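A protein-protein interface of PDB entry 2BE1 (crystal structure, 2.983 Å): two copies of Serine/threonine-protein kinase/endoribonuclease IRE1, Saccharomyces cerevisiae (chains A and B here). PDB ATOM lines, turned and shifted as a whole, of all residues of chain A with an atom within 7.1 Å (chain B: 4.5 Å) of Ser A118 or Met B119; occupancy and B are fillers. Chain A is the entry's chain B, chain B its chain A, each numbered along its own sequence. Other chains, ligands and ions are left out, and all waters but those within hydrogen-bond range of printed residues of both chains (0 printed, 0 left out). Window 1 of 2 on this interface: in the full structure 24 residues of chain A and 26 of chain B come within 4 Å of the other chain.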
ATOM      1  N   VAL A  89      -0.795   1.124 -16.662  1.00  0.00           N
ATOM      2  CA  VAL A  89      -1.690   1.388 -15.538  1.00  0.00           C
ATOM      3  C   VAL A  89      -3.029   1.959 -16.018  1.00  0.00           C
ATOM      4  O   VAL A  89      -4.085   1.574 -15.521  1.00  0.00           O
ATOM      5  CB  VAL A  89      -1.099   2.334 -14.488  1.00  0.00           C
ATOM      6  CG1 VAL A  89      -2.110   2.565 -13.413  1.00  0.00           C
ATOM      7  CG2 VAL A  89       0.189   1.758 -13.865  1.00  0.00           C
ATOM      8  N   SER A  90      -3.009   2.841 -17.015  1.00  0.00           N
ATOM      9  CA  SER A  90      -4.246   3.528 -17.416  1.00  0.00           C
ATOM     10  C   SER A  90      -5.103   2.635 -18.199  1.00  0.00           C
ATOM     11  O   SER A  90      -6.080   3.091 -18.731  1.00  0.00           O
ATOM     12  CB  SER A  90      -4.015   4.766 -18.298  1.00  0.00           C
ATOM     13  OG  SER A  90      -3.064   5.723 -17.759  1.00  0.00           O
ATOM     14  N   THR A  91      -4.742   1.376 -18.324  1.00  0.00           N
ATOM     15  CA  THR A  91      -5.623   0.496 -19.036  1.00  0.00           C
ATOM     16  C   THR A  91      -5.814  -0.812 -18.250  1.00  0.00           C
ATOM     17  O   THR A  91      -5.931  -1.908 -18.854  1.00  0.00           O
ATOM     18  CB  THR A  91      -5.202   0.318 -20.550  1.00  0.00           C
ATOM     19  OG1 THR A  91      -4.399  -0.852 -20.716  1.00  0.00           O
ATOM     20  CG2 THR A  91      -4.409   1.508 -21.062  1.00  0.00           C
ATOM     21  N   SER A  92      -5.850  -0.698 -16.913  1.00  0.00           N
ATOM     22  CA  SER A  92      -6.216  -1.827 -16.063  1.00  0.00           C
ATOM     23  C   SER A  92      -7.657  -1.705 -15.743  1.00  0.00           C
ATOM     24  O   SER A  92      -8.268  -0.722 -16.066  1.00  0.00           O
ATOM     25  CB  SER A  92      -5.535  -1.730 -14.752  1.00  0.00           C
ATOM     26  OG  SER A  92      -4.452  -0.907 -14.888  1.00  0.00           O
ATOM     27  N   THR A 116      -3.073  -5.371 -12.919  1.00  0.00           N
ATOM     28  CA  THR A 116      -3.742  -4.470 -12.003  1.00  0.00           C
ATOM     29  C   THR A 116      -2.836  -3.327 -11.631  1.00  0.00           C
ATOM     30  O   THR A 116      -1.713  -3.502 -11.157  1.00  0.00           O
ATOM     31  CB  THR A 116      -4.072  -5.152 -10.722  1.00  0.00           C
ATOM     32  OG1 THR A 116      -2.840  -5.484 -10.059  1.00  0.00           O
ATOM     33  CG2 THR A 116      -4.820  -6.425 -10.996  1.00  0.00           C
ATOM     34  N   GLY A 117      -3.376  -2.135 -11.779  1.00  0.00           N
ATOM     35  CA  GLY A 117      -2.608  -0.895 -11.598  1.00  0.00           C
ATOM     36  C   GLY A 117      -2.932  -0.132 -10.339  1.00  0.00           C
ATOM     37  O   GLY A 117      -3.610  -0.673  -9.434  1.00  0.00           O
ATOM     38  N   SER A 118      -2.437   1.112 -10.298  1.00  0.00           N
ATOM     39  CA  SER A 118      -2.472   1.967  -9.119  1.00  0.00           C
ATOM     40  C   SER A 118      -1.599   3.147  -9.427  1.00  0.00           C
ATOM     41  O   SER A 118      -0.440   3.002  -9.820  1.00  0.00           O
ATOM     42  CB  SER A 118      -1.976   1.214  -7.875  1.00  0.00           C
ATOM     43  OG  SER A 118      -1.141   1.956  -7.014  1.00  0.00           O
ATOM     44  N   MET A 119      -2.158   4.328  -9.235  1.00  0.00           N
ATOM     45  CA  MET A 119      -1.468   5.572  -9.452  1.00  0.00           C
ATOM     46  C   MET A 119      -1.849   6.548  -8.313  1.00  0.00           C
ATOM     47  O   MET A 119      -3.031   6.724  -8.020  1.00  0.00           O
ATOM     48  CB  MET A 119      -1.919   6.054 -10.814  1.00  0.00           C
ATOM     49  CG  MET A 119      -1.499   7.444 -11.142  1.00  0.00           C
ATOM     50  SD  MET A 119      -2.743   8.673 -10.659  1.00  0.00           S
ATOM     51  CE  MET A 119      -2.504   9.883 -11.995  1.00  0.00           C
ATOM     52  N   ARG A 120      -0.875   7.139  -7.639  1.00  0.00           N
ATOM     53  CA  ARG A 120      -1.194   8.129  -6.623  1.00  0.00           C
ATOM     54  C   ARG A 120      -0.606   9.437  -6.942  1.00  0.00           C
ATOM     55  O   ARG A 120       0.384   9.558  -7.641  1.00  0.00           O
ATOM     56  CB  ARG A 120      -0.553   7.839  -5.311  1.00  0.00           C
ATOM     57  CG  ARG A 120      -0.775   6.521  -4.790  1.00  0.00           C
ATOM     58  CD  ARG A 120      -0.387   6.502  -3.296  1.00  0.00           C
ATOM     59  NE  ARG A 120       1.061   6.473  -3.036  1.00  0.00           N
ATOM     60  CZ  ARG A 120       1.899   5.486  -3.425  1.00  0.00           C
ATOM     61  NH1 ARG A 120       3.199   5.601  -3.088  1.00  0.00           N
ATOM     62  NH2 ARG A 120       1.471   4.405  -4.158  1.00  0.00           N
ATOM     63  N   THR A 121      -1.147  10.432  -6.286  1.00  0.00           N
ATOM     64  CA  THR A 121      -0.659  11.782  -6.423  1.00  0.00           C
ATOM     65  C   THR A 121      -0.225  12.299  -5.026  1.00  0.00           C
ATOM     66  O   THR A 121      -0.789  11.869  -4.023  1.00  0.00           O
ATOM     67  CB  THR A 121      -1.795  12.567  -7.062  1.00  0.00           C
ATOM     68  OG1 THR A 121      -1.427  12.852  -8.402  1.00  0.00           O
ATOM     69  CG2 THR A 121      -2.045  13.825  -6.362  1.00  0.00           C
ATOM     70  N   ILE A 174       2.931   8.820  -8.567  1.00  0.00           N
ATOM     71  CA  ILE A 174       3.565   7.503  -8.346  1.00  0.00           C
ATOM     72  C   ILE A 174       2.765   6.315  -8.898  1.00  0.00           C
ATOM     73  O   ILE A 174       1.709   5.911  -8.345  1.00  0.00           O
ATOM     74  CB  ILE A 174       3.669   7.220  -6.876  1.00  0.00           C
ATOM     75  CG1 ILE A 174       4.474   8.317  -6.201  1.00  0.00           C
ATOM     76  CG2 ILE A 174       4.245   5.846  -6.637  1.00  0.00           C
ATOM     77  CD1 ILE A 174       4.247   8.411  -4.734  1.00  0.00           C
ATOM     78  N   PHE A 175       3.263   5.711  -9.966  1.00  0.00           N
ATOM     79  CA  PHE A 175       2.560   4.575 -10.541  1.00  0.00           C
ATOM     80  C   PHE A 175       3.026   3.275  -9.920  1.00  0.00           C
ATOM     81  O   PHE A 175       4.075   3.218  -9.232  1.00  0.00           O
ATOM     82  CB  PHE A 175       2.840   4.515 -12.016  1.00  0.00           C
ATOM     83  CG  PHE A 175       2.470   5.761 -12.746  1.00  0.00           C
ATOM     84  CD1 PHE A 175       3.255   6.892 -12.666  1.00  0.00           C
ATOM     85  CD2 PHE A 175       1.317   5.790 -13.527  1.00  0.00           C
ATOM     86  CE1 PHE A 175       2.890   8.026 -13.329  1.00  0.00           C
ATOM     87  CE2 PHE A 175       0.953   6.936 -14.194  1.00  0.00           C
ATOM     88  CZ  PHE A 175       1.742   8.045 -14.101  1.00  0.00           C
ATOM     89  N   GLU A 176       2.273   2.215 -10.197  1.00  0.00           N
ATOM     90  CA  GLU A 176       2.594   0.918  -9.636  1.00  0.00           C
ATOM     91  C   GLU A 176       1.857  -0.162 -10.345  1.00  0.00           C
ATOM     92  O   GLU A 176       0.728  -0.378 -10.072  1.00  0.00           O
ATOM     93  CB  GLU A 176       2.134   0.936  -8.224  1.00  0.00           C
ATOM     94  CG  GLU A 176       2.311  -0.320  -7.464  1.00  0.00           C
ATOM     95  CD  GLU A 176       1.976  -0.004  -6.014  1.00  0.00           C
ATOM     96  OE1 GLU A 176       0.773  -0.204  -5.604  1.00  0.00           O
ATOM     97  OE2 GLU A 176       2.911   0.536  -5.336  1.00  0.00           O
ATOM     98  N   LEU A 177       2.491  -0.831 -11.279  1.00  0.00           N
ATOM     99  CA  LEU A 177       1.831  -1.842 -12.100  1.00  0.00           C
ATOM    100  C   LEU A 177       2.177  -3.189 -11.522  1.00  0.00           C
ATOM    101  O   LEU A 177       3.297  -3.408 -11.096  1.00  0.00           O
ATOM    102  CB  LEU A 177       2.333  -1.765 -13.533  1.00  0.00           C
ATOM    103  CG  LEU A 177       1.733  -2.760 -14.499  1.00  0.00           C
ATOM    104  CD1 LEU A 177       0.756  -2.006 -15.376  1.00  0.00           C
ATOM    105  CD2 LEU A 177       2.771  -3.295 -15.357  1.00  0.00           C
ATOM    106  N   GLY A 178       1.208  -4.077 -11.470  1.00  0.00           N
ATOM    107  CA  GLY A 178       1.433  -5.358 -10.870  1.00  0.00           C
ATOM    108  C   GLY A 178       0.981  -6.267 -11.964  1.00  0.00           C
ATOM    109  O   GLY A 178      -0.153  -6.133 -12.435  1.00  0.00           O
ATOM    110  N   TYR A 191       6.910   2.893 -10.260  1.00  0.00           N
ATOM    111  CA  TYR A 191       7.654   3.919 -10.969  1.00  0.00           C
ATOM    112  C   TYR A 191       7.093   5.267 -10.587  1.00  0.00           C
ATOM    113  O   TYR A 191       5.930   5.566 -10.875  1.00  0.00           O
ATOM    114  CB  TYR A 191       7.505   3.732 -12.466  1.00  0.00           C
ATOM    115  CG  TYR A 191       7.723   5.028 -13.223  1.00  0.00           C
ATOM    116  CD1 TYR A 191       8.925   5.732 -13.129  1.00  0.00           C
ATOM    117  CD2 TYR A 191       6.727   5.564 -14.044  1.00  0.00           C
ATOM    118  CE1 TYR A 191       9.161   6.933 -13.882  1.00  0.00           C
ATOM    119  CE2 TYR A 191       6.938   6.769 -14.758  1.00  0.00           C
ATOM    120  CZ  TYR A 191       8.155   7.436 -14.677  1.00  0.00           C
ATOM    121  OH  TYR A 191       8.377   8.606 -15.364  1.00  0.00           O
ATOM    122  N   VAL B  89      -9.394  13.603  -9.679  1.00  0.00           N
ATOM    123  CA  VAL B  89      -8.234  12.794  -9.432  1.00  0.00           C
ATOM    124  C   VAL B  89      -7.273  12.901 -10.588  1.00  0.00           C
ATOM    125  O   VAL B  89      -6.083  13.014 -10.373  1.00  0.00           O
ATOM    126  CB  VAL B  89      -8.599  11.312  -9.276  1.00  0.00           C
ATOM    127  CG1 VAL B  89      -7.361  10.435  -9.358  1.00  0.00           C
ATOM    128  CG2 VAL B  89      -9.375  11.069  -7.961  1.00  0.00           C
ATOM    129  N   SER B 118      -5.652   9.592  -6.196  1.00  0.00           N
ATOM    130  CA  SER B 118      -5.277   8.220  -6.051  1.00  0.00           C
ATOM    131  C   SER B 118      -6.321   7.405  -6.732  1.00  0.00           C
ATOM    132  O   SER B 118      -7.536   7.571  -6.507  1.00  0.00           O
ATOM    133  CB  SER B 118      -5.157   7.883  -4.570  1.00  0.00           C
ATOM    134  OG  SER B 118      -5.651   6.610  -4.317  1.00  0.00           O
ATOM    135  N   MET B 119      -5.844   6.514  -7.573  1.00  0.00           N
ATOM    136  CA  MET B 119      -6.753   5.685  -8.303  1.00  0.00           C
ATOM    137  C   MET B 119      -6.208   4.278  -8.378  1.00  0.00           C
ATOM    138  O   MET B 119      -5.073   4.130  -8.773  1.00  0.00           O
ATOM    139  CB  MET B 119      -6.870   6.258  -9.689  1.00  0.00           C
ATOM    140  CG  MET B 119      -7.665   5.373 -10.592  1.00  0.00           C
ATOM    141  SD  MET B 119      -6.716   4.191 -11.570  1.00  0.00           S
ATOM    142  CE  MET B 119      -7.672   4.301 -13.106  1.00  0.00           C
ATOM    143  N   ARG B 120      -6.970   3.249  -8.001  1.00  0.00           N
ATOM    144  CA  ARG B 120      -6.450   1.862  -8.088  1.00  0.00           C
ATOM    145  C   ARG B 120      -7.274   0.964  -8.945  1.00  0.00           C
ATOM    146  O   ARG B 120      -8.494   1.058  -9.020  1.00  0.00           O
ATOM    147  CB  ARG B 120      -6.462   1.102  -6.768  1.00  0.00           C
ATOM    148  CG  ARG B 120      -5.911   1.739  -5.621  1.00  0.00           C
ATOM    149  CD  ARG B 120      -5.751   0.666  -4.556  1.00  0.00           C
ATOM    150  NE  ARG B 120      -6.975   0.259  -3.830  1.00  0.00           N
ATOM    151  CZ  ARG B 120      -7.794   1.075  -3.145  1.00  0.00           C
ATOM    152  NH1 ARG B 120      -8.843   0.527  -2.521  1.00  0.00           N
ATOM    153  NH2 ARG B 120      -7.607   2.433  -3.120  1.00  0.00           N
ATOM    154  N   THR B 121      -6.622  -0.065  -9.425  1.00  0.00           N
ATOM    155  CA  THR B 121      -7.316  -1.051 -10.196  1.00  0.00           C
ATOM    156  C   THR B 121      -7.272  -2.403  -9.429  1.00  0.00           C
ATOM    157  O   THR B 121      -6.272  -2.678  -8.710  1.00  0.00           O
ATOM    158  CB  THR B 121      -6.642  -1.023 -11.594  1.00  0.00           C
ATOM    159  OG1 THR B 121      -7.468  -0.265 -12.497  1.00  0.00           O
ATOM    160  CG2 THR B 121      -6.371  -2.414 -12.113  1.00  0.00           C
ATOM    161  N   PRO B 139      -3.490  -4.512  -6.054  1.00  0.00           N
ATOM    162  CA  PRO B 139      -3.409  -3.725  -4.823  1.00  0.00           C
ATOM    163  C   PRO B 139      -4.563  -3.948  -3.854  1.00  0.00           C
ATOM    164  O   PRO B 139      -4.992  -2.996  -3.204  1.00  0.00           O
ATOM    165  CB  PRO B 139      -3.439  -2.311  -5.368  1.00  0.00           C
ATOM    166  CG  PRO B 139      -2.571  -2.431  -6.621  1.00  0.00           C
ATOM    167  CD  PRO B 139      -2.638  -3.868  -7.088  1.00  0.00           C
ATOM    168  N   THR B 173     -12.404  -0.368 -10.588  1.00  0.00           N
ATOM    169  CA  THR B 173     -11.487   0.749 -10.344  1.00  0.00           C
ATOM    170  C   THR B 173     -11.918   1.531  -9.063  1.00  0.00           C
ATOM    171  O   THR B 173     -13.105   1.607  -8.751  1.00  0.00           O
ATOM    172  CB  THR B 173     -11.316   1.625 -11.628  1.00  0.00           C
ATOM    173  OG1 THR B 173     -10.951   2.952 -11.256  1.00  0.00           O
ATOM    174  CG2 THR B 173     -12.575   1.738 -12.449  1.00  0.00           C
ATOM    175  N   ILE B 174     -10.971   2.021  -8.280  1.00  0.00           N
ATOM    176  CA  ILE B 174     -11.307   2.713  -7.047  1.00  0.00           C
ATOM    177  C   ILE B 174     -10.558   4.000  -6.874  1.00  0.00           C
ATOM    178  O   ILE B 174      -9.338   4.016  -6.545  1.00  0.00           O
ATOM    179  CB  ILE B 174     -10.886   1.976  -5.845  1.00  0.00           C
ATOM    180  CG1 ILE B 174     -11.518   0.606  -5.825  1.00  0.00           C
ATOM    181  CG2 ILE B 174     -11.297   2.761  -4.654  1.00  0.00           C
ATOM    182  CD1 ILE B 174     -10.891  -0.318  -4.841  1.00  0.00           C
ATOM    183  N   PHE B 175     -11.304   5.088  -7.016  1.00  0.00           N
ATOM    184  CA  PHE B 175     -10.741   6.415  -6.913  1.00  0.00           C
ATOM    185  C   PHE B 175     -10.747   6.895  -5.476  1.00  0.00           C
ATOM    186  O   PHE B 175     -11.500   6.367  -4.615  1.00  0.00           O
ATOM    187  CB  PHE B 175     -11.598   7.373  -7.705  1.00  0.00           C
ATOM    188  CG  PHE B 175     -11.669   7.060  -9.136  1.00  0.00           C
ATOM    189  CD1 PHE B 175     -12.554   6.133  -9.592  1.00  0.00           C
ATOM    190  CD2 PHE B 175     -10.850   7.720 -10.051  1.00  0.00           C
ATOM    191  CE1 PHE B 175     -12.622   5.864 -10.933  1.00  0.00           C
ATOM    192  CE2 PHE B 175     -10.936   7.461 -11.396  1.00  0.00           C
ATOM    193  CZ  PHE B 175     -11.811   6.537 -11.830  1.00  0.00           C
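The backbone carbonyl oxygen (O) of Ser A118 sits at hydrogen-bond distance from the backbone NH (N) of Glu A176 (2.8 Å).
N of Gly A178 sits at hydrogen-bond distance from O of Thr A116.
OG of Ser A92 lies within hydrogen-bond range of O of Val A89, at 2.6 Å.
Of the 9 printed residues of chain B, 4 touch a printed residue of chain A.
Hydrophobic or aromatic side chains of chain B within 4 Å of the printed part of chain A: Pro B139.
Of the 16 printed residues of chain A, 5 touch a printed residue of chain B.
Printed residues of chain A that touch a printed residue of chain B: Ser A92, Thr A116, Gly A117, Ser A118 and Met A119.
Ser A118 touches just these residues of chain B: Met B119 (3.4 Å) and Pro B139 (3.9 Å).
Of the printed residues of chain A, Pro B139 touches Thr A116, Gly A117 and Ser A118.
Of the printed residues of chain A, Thr B121 touches Ser A92, Thr A116 and Gly A117.
Printed residues of chain B within 4 Å of Gly A117: Thr B121 and Pro B139.
Printed residues of chain B within 4 Å of Met A119: Ser B118 and Met B119.
Phe B175 touches none of the printed residues of chain A.
The nearest residue of chain B that does not touch Ser A118 is Arg B120 (4.1 Å).
The nearest printed residue of chain A that does not touch Met B119 is Arg A120 (5.0 Å).
N of Thr B121 lies within hydrogen-bond range of O of Gly A117, 3.1 Å away.
The backbone NH (N) of Met B119 is in hydrogen-bond range of the backbone carbonyl oxygen (O) of Met A119, 2.9 Å away.
Ser A118 touches Met B119, and with the chains exchanged Met A119 touches Ser B118.
Met A119 touches its own counterpart, Met B119.
7 positions are printed for both chains.
Of the 9 pairs that touch across the chains among the printed residues, 3 have their exchanged pair printed and touching as well.
Among the printed residues, pairs that only touch across the chains: Ser A92 with Thr B121, Thr A116 with Thr B121, Thr A116 with Pro B139, Gly A117 with Pro B139, Ser A118 with Met B119, Ser A118 with Pro B139 and Met A119 with Ser B118.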
